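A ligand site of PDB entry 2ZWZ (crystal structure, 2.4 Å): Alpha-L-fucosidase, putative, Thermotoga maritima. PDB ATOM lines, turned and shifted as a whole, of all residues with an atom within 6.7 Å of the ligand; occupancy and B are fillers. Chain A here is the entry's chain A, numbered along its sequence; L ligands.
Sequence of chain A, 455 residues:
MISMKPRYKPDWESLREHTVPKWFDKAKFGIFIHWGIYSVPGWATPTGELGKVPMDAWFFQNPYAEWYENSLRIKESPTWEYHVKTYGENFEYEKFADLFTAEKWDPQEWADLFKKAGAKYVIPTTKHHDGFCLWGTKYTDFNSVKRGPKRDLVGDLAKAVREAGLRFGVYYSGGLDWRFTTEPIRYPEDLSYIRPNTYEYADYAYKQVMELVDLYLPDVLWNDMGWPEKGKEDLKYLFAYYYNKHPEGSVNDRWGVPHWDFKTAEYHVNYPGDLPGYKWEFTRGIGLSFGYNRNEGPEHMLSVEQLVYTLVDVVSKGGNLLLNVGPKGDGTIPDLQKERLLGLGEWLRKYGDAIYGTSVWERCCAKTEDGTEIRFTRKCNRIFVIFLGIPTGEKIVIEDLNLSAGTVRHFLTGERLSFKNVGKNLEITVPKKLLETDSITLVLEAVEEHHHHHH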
ATOM      1  N   PHE A  32     -28.778 -21.808 -17.376  1.00  0.00           N
ATOM      2  CA  PHE A  32     -28.054 -20.642 -16.909  1.00  0.00           C
ATOM      3  C   PHE A  32     -27.523 -19.866 -18.142  1.00  0.00           C
ATOM      4  O   PHE A  32     -27.114 -20.461 -19.126  1.00  0.00           O
ATOM      5  CB  PHE A  32     -26.817 -21.082 -16.118  1.00  0.00           C
ATOM      6  CG  PHE A  32     -26.602 -20.352 -14.828  1.00  0.00           C
ATOM      7  CD1 PHE A  32     -27.380 -19.224 -14.474  1.00  0.00           C
ATOM      8  CD2 PHE A  32     -25.625 -20.813 -13.910  1.00  0.00           C
ATOM      9  CE1 PHE A  32     -27.189 -18.572 -13.223  1.00  0.00           C
ATOM     10  CE2 PHE A  32     -25.429 -20.222 -12.712  1.00  0.00           C
ATOM     11  CZ  PHE A  32     -26.211 -19.079 -12.347  1.00  0.00           C
ATOM     12  N   HIS A  34     -24.709 -16.873 -18.823  1.00  0.00           N
ATOM     13  CA  HIS A  34     -23.719 -15.867 -18.520  1.00  0.00           C
ATOM     14  C   HIS A  34     -23.398 -15.134 -19.834  1.00  0.00           C
ATOM     15  O   HIS A  34     -22.674 -15.594 -20.728  1.00  0.00           O
ATOM     16  CB  HIS A  34     -22.498 -16.494 -17.876  1.00  0.00           C
ATOM     17  CG  HIS A  34     -22.699 -16.773 -16.410  1.00  0.00           C
ATOM     18  ND1 HIS A  34     -23.708 -17.613 -15.944  1.00  0.00           N
ATOM     19  CD2 HIS A  34     -22.038 -16.341 -15.309  1.00  0.00           C
ATOM     20  CE1 HIS A  34     -23.650 -17.676 -14.621  1.00  0.00           C
ATOM     21  NE2 HIS A  34     -22.645 -16.918 -14.217  1.00  0.00           N
ATOM     22  N   LEU A  50     -13.353 -25.870 -11.436  1.00  0.00           N
ATOM     23  CA  LEU A  50     -13.324 -25.330 -10.072  1.00  0.00           C
ATOM     24  C   LEU A  50     -13.306 -26.507  -9.076  1.00  0.00           C
ATOM     25  O   LEU A  50     -14.135 -27.426  -9.161  1.00  0.00           O
ATOM     26  CB  LEU A  50     -14.578 -24.471  -9.794  1.00  0.00           C
ATOM     27  CG  LEU A  50     -14.545 -23.710  -8.465  1.00  0.00           C
ATOM     28  CD1 LEU A  50     -13.439 -22.628  -8.511  1.00  0.00           C
ATOM     29  CD2 LEU A  50     -15.889 -23.092  -8.187  1.00  0.00           C
ATOM     30  N   TYR A  64     -12.731 -19.005 -16.096  1.00  0.00           N
ATOM     31  CA  TYR A  64     -14.008 -18.337 -16.255  1.00  0.00           C
ATOM     32  C   TYR A  64     -13.812 -17.104 -17.114  1.00  0.00           C
ATOM     33  O   TYR A  64     -13.266 -16.074 -16.670  1.00  0.00           O
ATOM     34  CB  TYR A  64     -14.569 -17.904 -14.917  1.00  0.00           C
ATOM     35  CG  TYR A  64     -15.078 -19.046 -14.045  1.00  0.00           C
ATOM     36  CD1 TYR A  64     -15.006 -20.400 -14.487  1.00  0.00           C
ATOM     37  CD2 TYR A  64     -15.697 -18.759 -12.802  1.00  0.00           C
ATOM     38  CE1 TYR A  64     -15.555 -21.465 -13.671  1.00  0.00           C
ATOM     39  CE2 TYR A  64     -16.245 -19.767 -11.997  1.00  0.00           C
ATOM     40  CZ  TYR A  64     -16.183 -21.123 -12.439  1.00  0.00           C
ATOM     41  OH  TYR A  64     -16.757 -22.046 -11.625  1.00  0.00           O
ATOM     42  N   GLU A  66     -15.871 -15.004 -17.941  1.00  0.00           N
ATOM     43  CA  GLU A  66     -16.593 -13.844 -17.471  1.00  0.00           C
ATOM     44  C   GLU A  66     -15.785 -13.002 -16.454  1.00  0.00           C
ATOM     45  O   GLU A  66     -16.160 -11.843 -16.118  1.00  0.00           O
ATOM     46  CB  GLU A  66     -17.958 -14.229 -16.872  1.00  0.00           C
ATOM     47  CG  GLU A  66     -17.973 -15.024 -15.562  1.00  0.00           C
ATOM     48  CD  GLU A  66     -17.616 -16.506 -15.715  1.00  0.00           C
ATOM     49  OE1 GLU A  66     -17.710 -17.280 -14.736  1.00  0.00           O
ATOM     50  OE2 GLU A  66     -17.233 -16.898 -16.827  1.00  0.00           O
ATOM     51  N   TRP A  67     -14.665 -13.555 -15.974  1.00  0.00           N
ATOM     52  CA  TRP A  67     -13.775 -12.855 -15.028  1.00  0.00           C
ATOM     53  C   TRP A  67     -12.694 -12.070 -15.773  1.00  0.00           C
ATOM     54  O   TRP A  67     -11.709 -11.632 -15.172  1.00  0.00           O
ATOM     55  CB  TRP A  67     -13.061 -13.822 -14.051  1.00  0.00           C
ATOM     56  CG  TRP A  67     -13.912 -14.232 -12.816  1.00  0.00           C
ATOM     57  CD1 TRP A  67     -15.106 -14.908 -12.822  1.00  0.00           C
ATOM     58  CD2 TRP A  67     -13.651 -13.905 -11.458  1.00  0.00           C
ATOM     59  NE1 TRP A  67     -15.597 -15.002 -11.571  1.00  0.00           N
ATOM     60  CE2 TRP A  67     -14.735 -14.394 -10.698  1.00  0.00           C
ATOM     61  CE3 TRP A  67     -12.599 -13.234 -10.814  1.00  0.00           C
ATOM     62  CZ2 TRP A  67     -14.823 -14.235  -9.318  1.00  0.00           C
ATOM     63  CZ3 TRP A  67     -12.685 -13.078  -9.449  1.00  0.00           C
ATOM     64  CH2 TRP A  67     -13.807 -13.583  -8.697  1.00  0.00           C
ATOM     65  N   THR A 125     -27.803 -13.716 -16.443  1.00  0.00           N
ATOM     66  CA  THR A 125     -27.017 -12.827 -15.633  1.00  0.00           C
ATOM     67  C   THR A 125     -27.550 -11.425 -15.898  1.00  0.00           C
ATOM     68  O   THR A 125     -27.362 -10.905 -16.977  1.00  0.00           O
ATOM     69  CB  THR A 125     -25.482 -12.919 -16.027  1.00  0.00           C
ATOM     70  OG1 THR A 125     -25.362 -12.887 -17.461  1.00  0.00           O
ATOM     71  CG2 THR A 125     -24.826 -14.215 -15.493  1.00  0.00           C
ATOM     72  N   HIS A 128     -23.374  -9.238 -13.733  1.00  0.00           N
ATOM     73  CA  HIS A 128     -22.310 -10.065 -13.228  1.00  0.00           C
ATOM     74  C   HIS A 128     -21.285  -9.193 -12.438  1.00  0.00           C
ATOM     75  O   HIS A 128     -21.522  -8.007 -12.113  1.00  0.00           O
ATOM     76  CB  HIS A 128     -21.646 -10.841 -14.329  1.00  0.00           C
ATOM     77  CG  HIS A 128     -20.996 -12.088 -13.834  1.00  0.00           C
ATOM     78  ND1 HIS A 128     -19.632 -12.186 -13.601  1.00  0.00           N
ATOM     79  CD2 HIS A 128     -21.529 -13.278 -13.449  1.00  0.00           C
ATOM     80  CE1 HIS A 128     -19.370 -13.375 -13.089  1.00  0.00           C
ATOM     81  NE2 HIS A 128     -20.492 -14.051 -12.979  1.00  0.00           N
ATOM     82  N   HIS A 129     -20.162  -9.771 -12.083  1.00  0.00           N
ATOM     83  CA  HIS A 129     -19.180  -9.059 -11.289  1.00  0.00           C
ATOM     84  C   HIS A 129     -18.664  -7.744 -11.866  1.00  0.00           C
ATOM     85  O   HIS A 129     -18.278  -6.884 -11.096  1.00  0.00           O
ATOM     86  CB  HIS A 129     -17.963  -9.960 -11.006  1.00  0.00           C
ATOM     87  CG  HIS A 129     -18.312 -11.298 -10.426  1.00  0.00           C
ATOM     88  ND1 HIS A 129     -19.501 -11.551  -9.781  1.00  0.00           N
ATOM     89  CD2 HIS A 129     -17.623 -12.472 -10.448  1.00  0.00           C
ATOM     90  CE1 HIS A 129     -19.544 -12.834  -9.453  1.00  0.00           C
ATOM     91  NE2 HIS A 129     -18.421 -13.416  -9.843  1.00  0.00           N
ATOM     92  N   TYR A 171     -30.236 -13.838 -12.249  1.00  0.00           N
ATOM     93  CA  TYR A 171     -28.966 -13.957 -11.559  1.00  0.00           C
ATOM     94  C   TYR A 171     -28.524 -12.497 -11.282  1.00  0.00           C
ATOM     95  O   TYR A 171     -28.628 -11.621 -12.187  1.00  0.00           O
ATOM     96  CB  TYR A 171     -27.926 -14.646 -12.460  1.00  0.00           C
ATOM     97  CG  TYR A 171     -26.515 -14.507 -11.942  1.00  0.00           C
ATOM     98  CD1 TYR A 171     -25.890 -15.560 -11.306  1.00  0.00           C
ATOM     99  CD2 TYR A 171     -25.803 -13.290 -12.087  1.00  0.00           C
ATOM    100  CE1 TYR A 171     -24.588 -15.419 -10.829  1.00  0.00           C
ATOM    101  CE2 TYR A 171     -24.523 -13.138 -11.615  1.00  0.00           C
ATOM    102  CZ  TYR A 171     -23.916 -14.198 -10.994  1.00  0.00           C
ATOM    103  OH  TYR A 171     -22.636 -14.083 -10.558  1.00  0.00           O
ATOM    104  N   LEU A 176     -20.167  -9.009  -5.571  1.00  0.00           N
ATOM    105  CA  LEU A 176     -19.046  -8.368  -6.233  1.00  0.00           C
ATOM    106  C   LEU A 176     -19.550  -7.385  -7.327  1.00  0.00           C
ATOM    107  O   LEU A 176     -20.567  -7.615  -7.993  1.00  0.00           O
ATOM    108  CB  LEU A 176     -18.156  -9.464  -6.906  1.00  0.00           C
ATOM    109  CG  LEU A 176     -17.418 -10.575  -6.144  1.00  0.00           C
ATOM    110  CD1 LEU A 176     -16.580 -11.519  -7.135  1.00  0.00           C
ATOM    111  CD2 LEU A 176     -16.454  -9.931  -5.107  1.00  0.00           C
ATOM    112  N   TRP A 222     -31.418 -15.470  -7.875  1.00  0.00           N
ATOM    113  CA  TRP A 222     -30.205 -16.269  -7.764  1.00  0.00           C
ATOM    114  C   TRP A 222     -29.060 -15.304  -7.529  1.00  0.00           C
ATOM    115  O   TRP A 222     -28.469 -14.765  -8.478  1.00  0.00           O
ATOM    116  CB  TRP A 222     -30.008 -17.076  -9.072  1.00  0.00           C
ATOM    117  CG  TRP A 222     -29.272 -18.403  -8.957  1.00  0.00           C
ATOM    118  CD1 TRP A 222     -29.851 -19.644  -9.024  1.00  0.00           C
ATOM    119  CD2 TRP A 222     -27.856 -18.636  -8.816  1.00  0.00           C
ATOM    120  NE1 TRP A 222     -28.888 -20.639  -8.926  1.00  0.00           N
ATOM    121  CE2 TRP A 222     -27.658 -20.049  -8.797  1.00  0.00           C
ATOM    122  CE3 TRP A 222     -26.722 -17.787  -8.705  1.00  0.00           C
ATOM    123  CZ2 TRP A 222     -26.391 -20.641  -8.684  1.00  0.00           C
ATOM    124  CZ3 TRP A 222     -25.478 -18.361  -8.590  1.00  0.00           C
ATOM    125  CH2 TRP A 222     -25.315 -19.802  -8.577  1.00  0.00           C
ATOM    126  N   ASP A 224     -25.225 -14.113  -6.153  1.00  0.00           N
ATOM    127  CA  ASP A 224     -23.936 -14.767  -6.177  1.00  0.00           C
ATOM    128  C   ASP A 224     -22.978 -13.965  -5.287  1.00  0.00           C
ATOM    129  O   ASP A 224     -23.156 -12.750  -5.114  1.00  0.00           O
ATOM    130  CB  ASP A 224     -23.401 -14.836  -7.610  1.00  0.00           C
ATOM    131  CG  ASP A 224     -22.398 -15.970  -7.821  1.00  0.00           C
ATOM    132  OD1 ASP A 224     -21.902 -16.134  -8.943  1.00  0.00           O
ATOM    133  OD2 ASP A 224     -22.101 -16.701  -6.864  1.00  0.00           O
ATOM    134  N   MET A 225     -22.032 -14.683  -4.694  1.00  0.00           N
ATOM    135  CA  MET A 225     -20.961 -14.126  -3.910  1.00  0.00           C
ATOM    136  C   MET A 225     -21.278 -13.448  -2.599  1.00  0.00           C
ATOM    137  O   MET A 225     -20.534 -12.633  -2.112  1.00  0.00           O
ATOM    138  CB  MET A 225     -20.123 -13.200  -4.840  1.00  0.00           C
ATOM    139  CG  MET A 225     -19.305 -14.021  -5.857  1.00  0.00           C
ATOM    140  SD  MET A 225     -17.966 -14.918  -4.952  1.00  0.00           S
ATOM    141  CE  MET A 225     -16.599 -15.116  -6.309  1.00  0.00           C
ATOM    142  N   ARG A 254     -26.884 -18.097  -1.541  1.00  0.00           N
ATOM    143  CA  ARG A 254     -25.642 -17.371  -1.611  1.00  0.00           C
ATOM    144  C   ARG A 254     -25.773 -15.931  -1.135  1.00  0.00           C
ATOM    145  O   ARG A 254     -25.163 -15.029  -1.724  1.00  0.00           O
ATOM    146  CB  ARG A 254     -25.148 -17.383  -3.053  1.00  0.00           C
ATOM    147  CG  ARG A 254     -24.975 -18.766  -3.673  1.00  0.00           C
ATOM    148  CD  ARG A 254     -24.090 -18.769  -4.919  1.00  0.00           C
ATOM    149  NE  ARG A 254     -23.764 -20.154  -5.282  1.00  0.00           N
ATOM    150  CZ  ARG A 254     -22.837 -20.504  -6.159  1.00  0.00           C
ATOM    151  NH1 ARG A 254     -22.588 -21.792  -6.420  1.00  0.00           N
ATOM    152  NH2 ARG A 254     -22.158 -19.564  -6.799  1.00  0.00           N
ATOM    153  N   GLU A 266     -21.244 -25.823  -7.274  1.00  0.00           N
ATOM    154  CA  GLU A 266     -20.631 -25.333  -8.508  1.00  0.00           C
ATOM    155  C   GLU A 266     -19.407 -26.266  -8.870  1.00  0.00           C
ATOM    156  O   GLU A 266     -18.450 -26.372  -8.125  1.00  0.00           O
ATOM    157  CB  GLU A 266     -20.258 -23.868  -8.262  1.00  0.00           C
ATOM    158  CG  GLU A 266     -19.655 -23.134  -9.406  1.00  0.00           C
ATOM    159  CD  GLU A 266     -19.604 -21.644  -9.143  1.00  0.00           C
ATOM    160  OE1 GLU A 266     -18.678 -20.995  -9.684  1.00  0.00           O
ATOM    161  OE2 GLU A 266     -20.489 -21.116  -8.426  1.00  0.00           O
ATOM    162  N   THR A 283     -24.652 -26.475 -10.588  1.00  0.00           N
ATOM    163  CA  THR A 283     -24.433 -25.638 -11.746  1.00  0.00           C
ATOM    164  C   THR A 283     -22.980 -25.785 -12.269  1.00  0.00           C
ATOM    165  O   THR A 283     -22.018 -26.088 -11.521  1.00  0.00           O
ATOM    166  CB  THR A 283     -24.761 -24.161 -11.429  1.00  0.00           C
ATOM    167  OG1 THR A 283     -24.953 -23.453 -12.645  1.00  0.00           O
ATOM    168  CG2 THR A 283     -23.629 -23.462 -10.710  1.00  0.00           C
ATOM    169  N   ARG A 284     -22.858 -25.594 -13.574  1.00  0.00           N
ATOM    170  CA  ARG A 284     -21.584 -25.662 -14.314  1.00  0.00           C
ATOM    171  C   ARG A 284     -21.852 -25.226 -15.754  1.00  0.00           C
ATOM    172  O   ARG A 284     -23.028 -25.167 -16.212  1.00  0.00           O
ATOM    173  CB  ARG A 284     -21.000 -27.094 -14.371  1.00  0.00           C
ATOM    174  CG  ARG A 284     -21.851 -28.158 -15.126  1.00  0.00           C
ATOM    175  CD  ARG A 284     -21.019 -29.400 -15.509  1.00  0.00           C
ATOM    176  NE  ARG A 284     -19.999 -28.971 -16.475  1.00  0.00           N
ATOM    177  CZ  ARG A 284     -18.850 -29.587 -16.733  1.00  0.00           C
ATOM    178  NH1 ARG A 284     -18.552 -30.693 -16.095  1.00  0.00           N
ATOM    179  NH2 ARG A 284     -18.014 -29.067 -17.643  1.00  0.00           N
ATOM    180  N   PHE A 290     -18.199 -19.997 -17.748  1.00  0.00           N
ATOM    181  CA  PHE A 290     -19.623 -19.692 -17.817  1.00  0.00           C
ATOM    182  C   PHE A 290     -19.800 -18.781 -19.019  1.00  0.00           C
ATOM    183  O   PHE A 290     -20.606 -19.029 -19.861  1.00  0.00           O
ATOM    184  CB  PHE A 290     -20.157 -19.113 -16.504  1.00  0.00           C
ATOM    185  CG  PHE A 290     -20.314 -20.138 -15.448  1.00  0.00           C
ATOM    186  CD1 PHE A 290     -19.210 -20.562 -14.690  1.00  0.00           C
ATOM    187  CD2 PHE A 290     -21.563 -20.689 -15.166  1.00  0.00           C
ATOM    188  CE1 PHE A 290     -19.371 -21.497 -13.659  1.00  0.00           C
ATOM    189  CE2 PHE A 290     -21.725 -21.624 -14.135  1.00  0.00           C
ATOM    190  CZ  PHE A 290     -20.642 -22.038 -13.381  1.00  0.00           C
ATOM    191  N   GLY A 291     -19.000 -17.747 -19.097  1.00  0.00           N
ATOM    192  CA  GLY A 291     -19.083 -16.876 -20.245  1.00  0.00           C
ATOM    193  C   GLY A 291     -18.395 -17.586 -21.400  1.00  0.00           C
ATOM    194  O   GLY A 291     -17.528 -18.487 -21.200  1.00  0.00           O
ATOM    195  N   ASN A 324     -25.156 -24.097 -17.704  1.00  0.00           N
ATOM    196  CA  ASN A 324     -24.838 -22.820 -18.275  1.00  0.00           C
ATOM    197  C   ASN A 324     -24.530 -22.792 -19.767  1.00  0.00           C
ATOM    198  O   ASN A 324     -23.799 -23.633 -20.290  1.00  0.00           O
ATOM    199  CB  ASN A 324     -23.632 -22.195 -17.547  1.00  0.00           C
ATOM    200  CG  ASN A 324     -23.265 -20.803 -18.092  1.00  0.00           C
ATOM    201  OD1 ASN A 324     -23.914 -19.811 -17.784  1.00  0.00           O
ATOM    202  ND2 ASN A 324     -22.220 -20.740 -18.941  1.00  0.00           N
HETATM  203  O1  LIG L   1     -17.605 -16.174  -9.980  1.00  0.00           O
HETATM  204  C1  LIG L   1     -18.868 -16.770 -10.315  1.00  0.00           C
HETATM  205  C2  LIG L   1     -18.850 -17.249 -11.771  1.00  0.00           C
HETATM  206  O2  LIG L   1     -18.501 -16.178 -12.647  1.00  0.00           O
HETATM  207  C3  LIG L   1     -20.251 -17.750 -12.110  1.00  0.00           C
HETATM  208  O3  LIG L   1     -21.140 -16.630 -12.021  1.00  0.00           O
HETATM  209  C4  LIG L   1     -20.653 -18.858 -11.124  1.00  0.00           C
HETATM  210  C5  LIG L   1     -22.073 -19.353 -11.387  1.00  0.00           C
HETATM  211  N1  LIG L   1     -20.561 -18.402  -9.723  1.00  0.00           N
HETATM  212  C6  LIG L   1     -19.200 -17.953  -9.393  1.00  0.00           C
HETATM  213  C7  LIG L   1     -19.157 -17.542  -7.924  1.00  0.00           C
HETATM  214  N2  LIG L   1     -18.996 -18.723  -7.056  1.00  0.00           N
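OE1 of Glu 66 is in hydrogen-bond range of O2 of the ligand. A ring nitrogen (NE2) of His 34 lies within hydrogen-bond range of an oxygen (O3) of the ligand, 2.7 Å away. OD1 of Asp 224 is in salt-bridge range of N1 of the ligand. The indole nitrogen (NE1) of Trp 67 is in hydrogen-bond range of an oxygen (O1) of the ligand (2.8 Å). NE2 of His 128 lies within hydrogen-bond range of O3 of the ligand (2.8 Å). A ring nitrogen (NE2) of His 129 is in hydrogen-bond range of an oxygen (O1) of the ligand (2.9 Å). The side-chain carboxylate (OE2) of Glu 266 is in salt-bridge range of a nitrogen (N1) of the ligand (3.0 Å). NH2 of Arg 254 sits close to N2 of the ligand (3.3 Å). OH of Tyr 171 is in hydrogen-bond range of O3 of the ligand (3.3 Å).
Phe 32 touches the ligand (CE2 to C5, 3.7 Å). CE2 of Tyr 64 touches C2 of the ligand (3.6 Å). Met 225 touches the ligand. Phe 290 touches the ligand (CE2 to C5, 3.6 Å). Hydrophobic or aromatic side chains within 4 Å of the ligand: Phe 32, His 34, Tyr 64, Trp 67, His 128, His 129, Tyr 171, Met 225 and Phe 290. The nearest printed residue that does not touch the ligand is Trp 222 (4.3 Å).
The side-chain carboxylate (OE2) of Glu 66 is in hydrogen-bond range of the backbone NH (N) of Phe 290, 3.4 Å away. The backbone NH of Gly 291 is in hydrogen-bond range of the side-chain carboxylate of Glu 66 (3.0 Å). A ring nitrogen (ND1) of His 34 is in hydrogen-bond range of the side-chain amide oxygen (OD1) of Asn 324 (2.9 Å). The guanidinium group of Arg 254 is in salt-bridge range of the side-chain carboxylate of Asp 224 (2.9 Å). A ring nitrogen (NE2) of His 128 sits close to the side-chain hydroxyl of Tyr 171, 3.2 Å away. NH2 of Arg 254 is in salt-bridge range of OE2 of Glu 266. OH of Tyr 64 sits at hydrogen-bond distance from OE1 of Glu 266. The backbone carbonyl oxygen of Phe 290 is in hydrogen-bond range of the side-chain amide nitrogen of Asn 324, 2.5 Å away.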
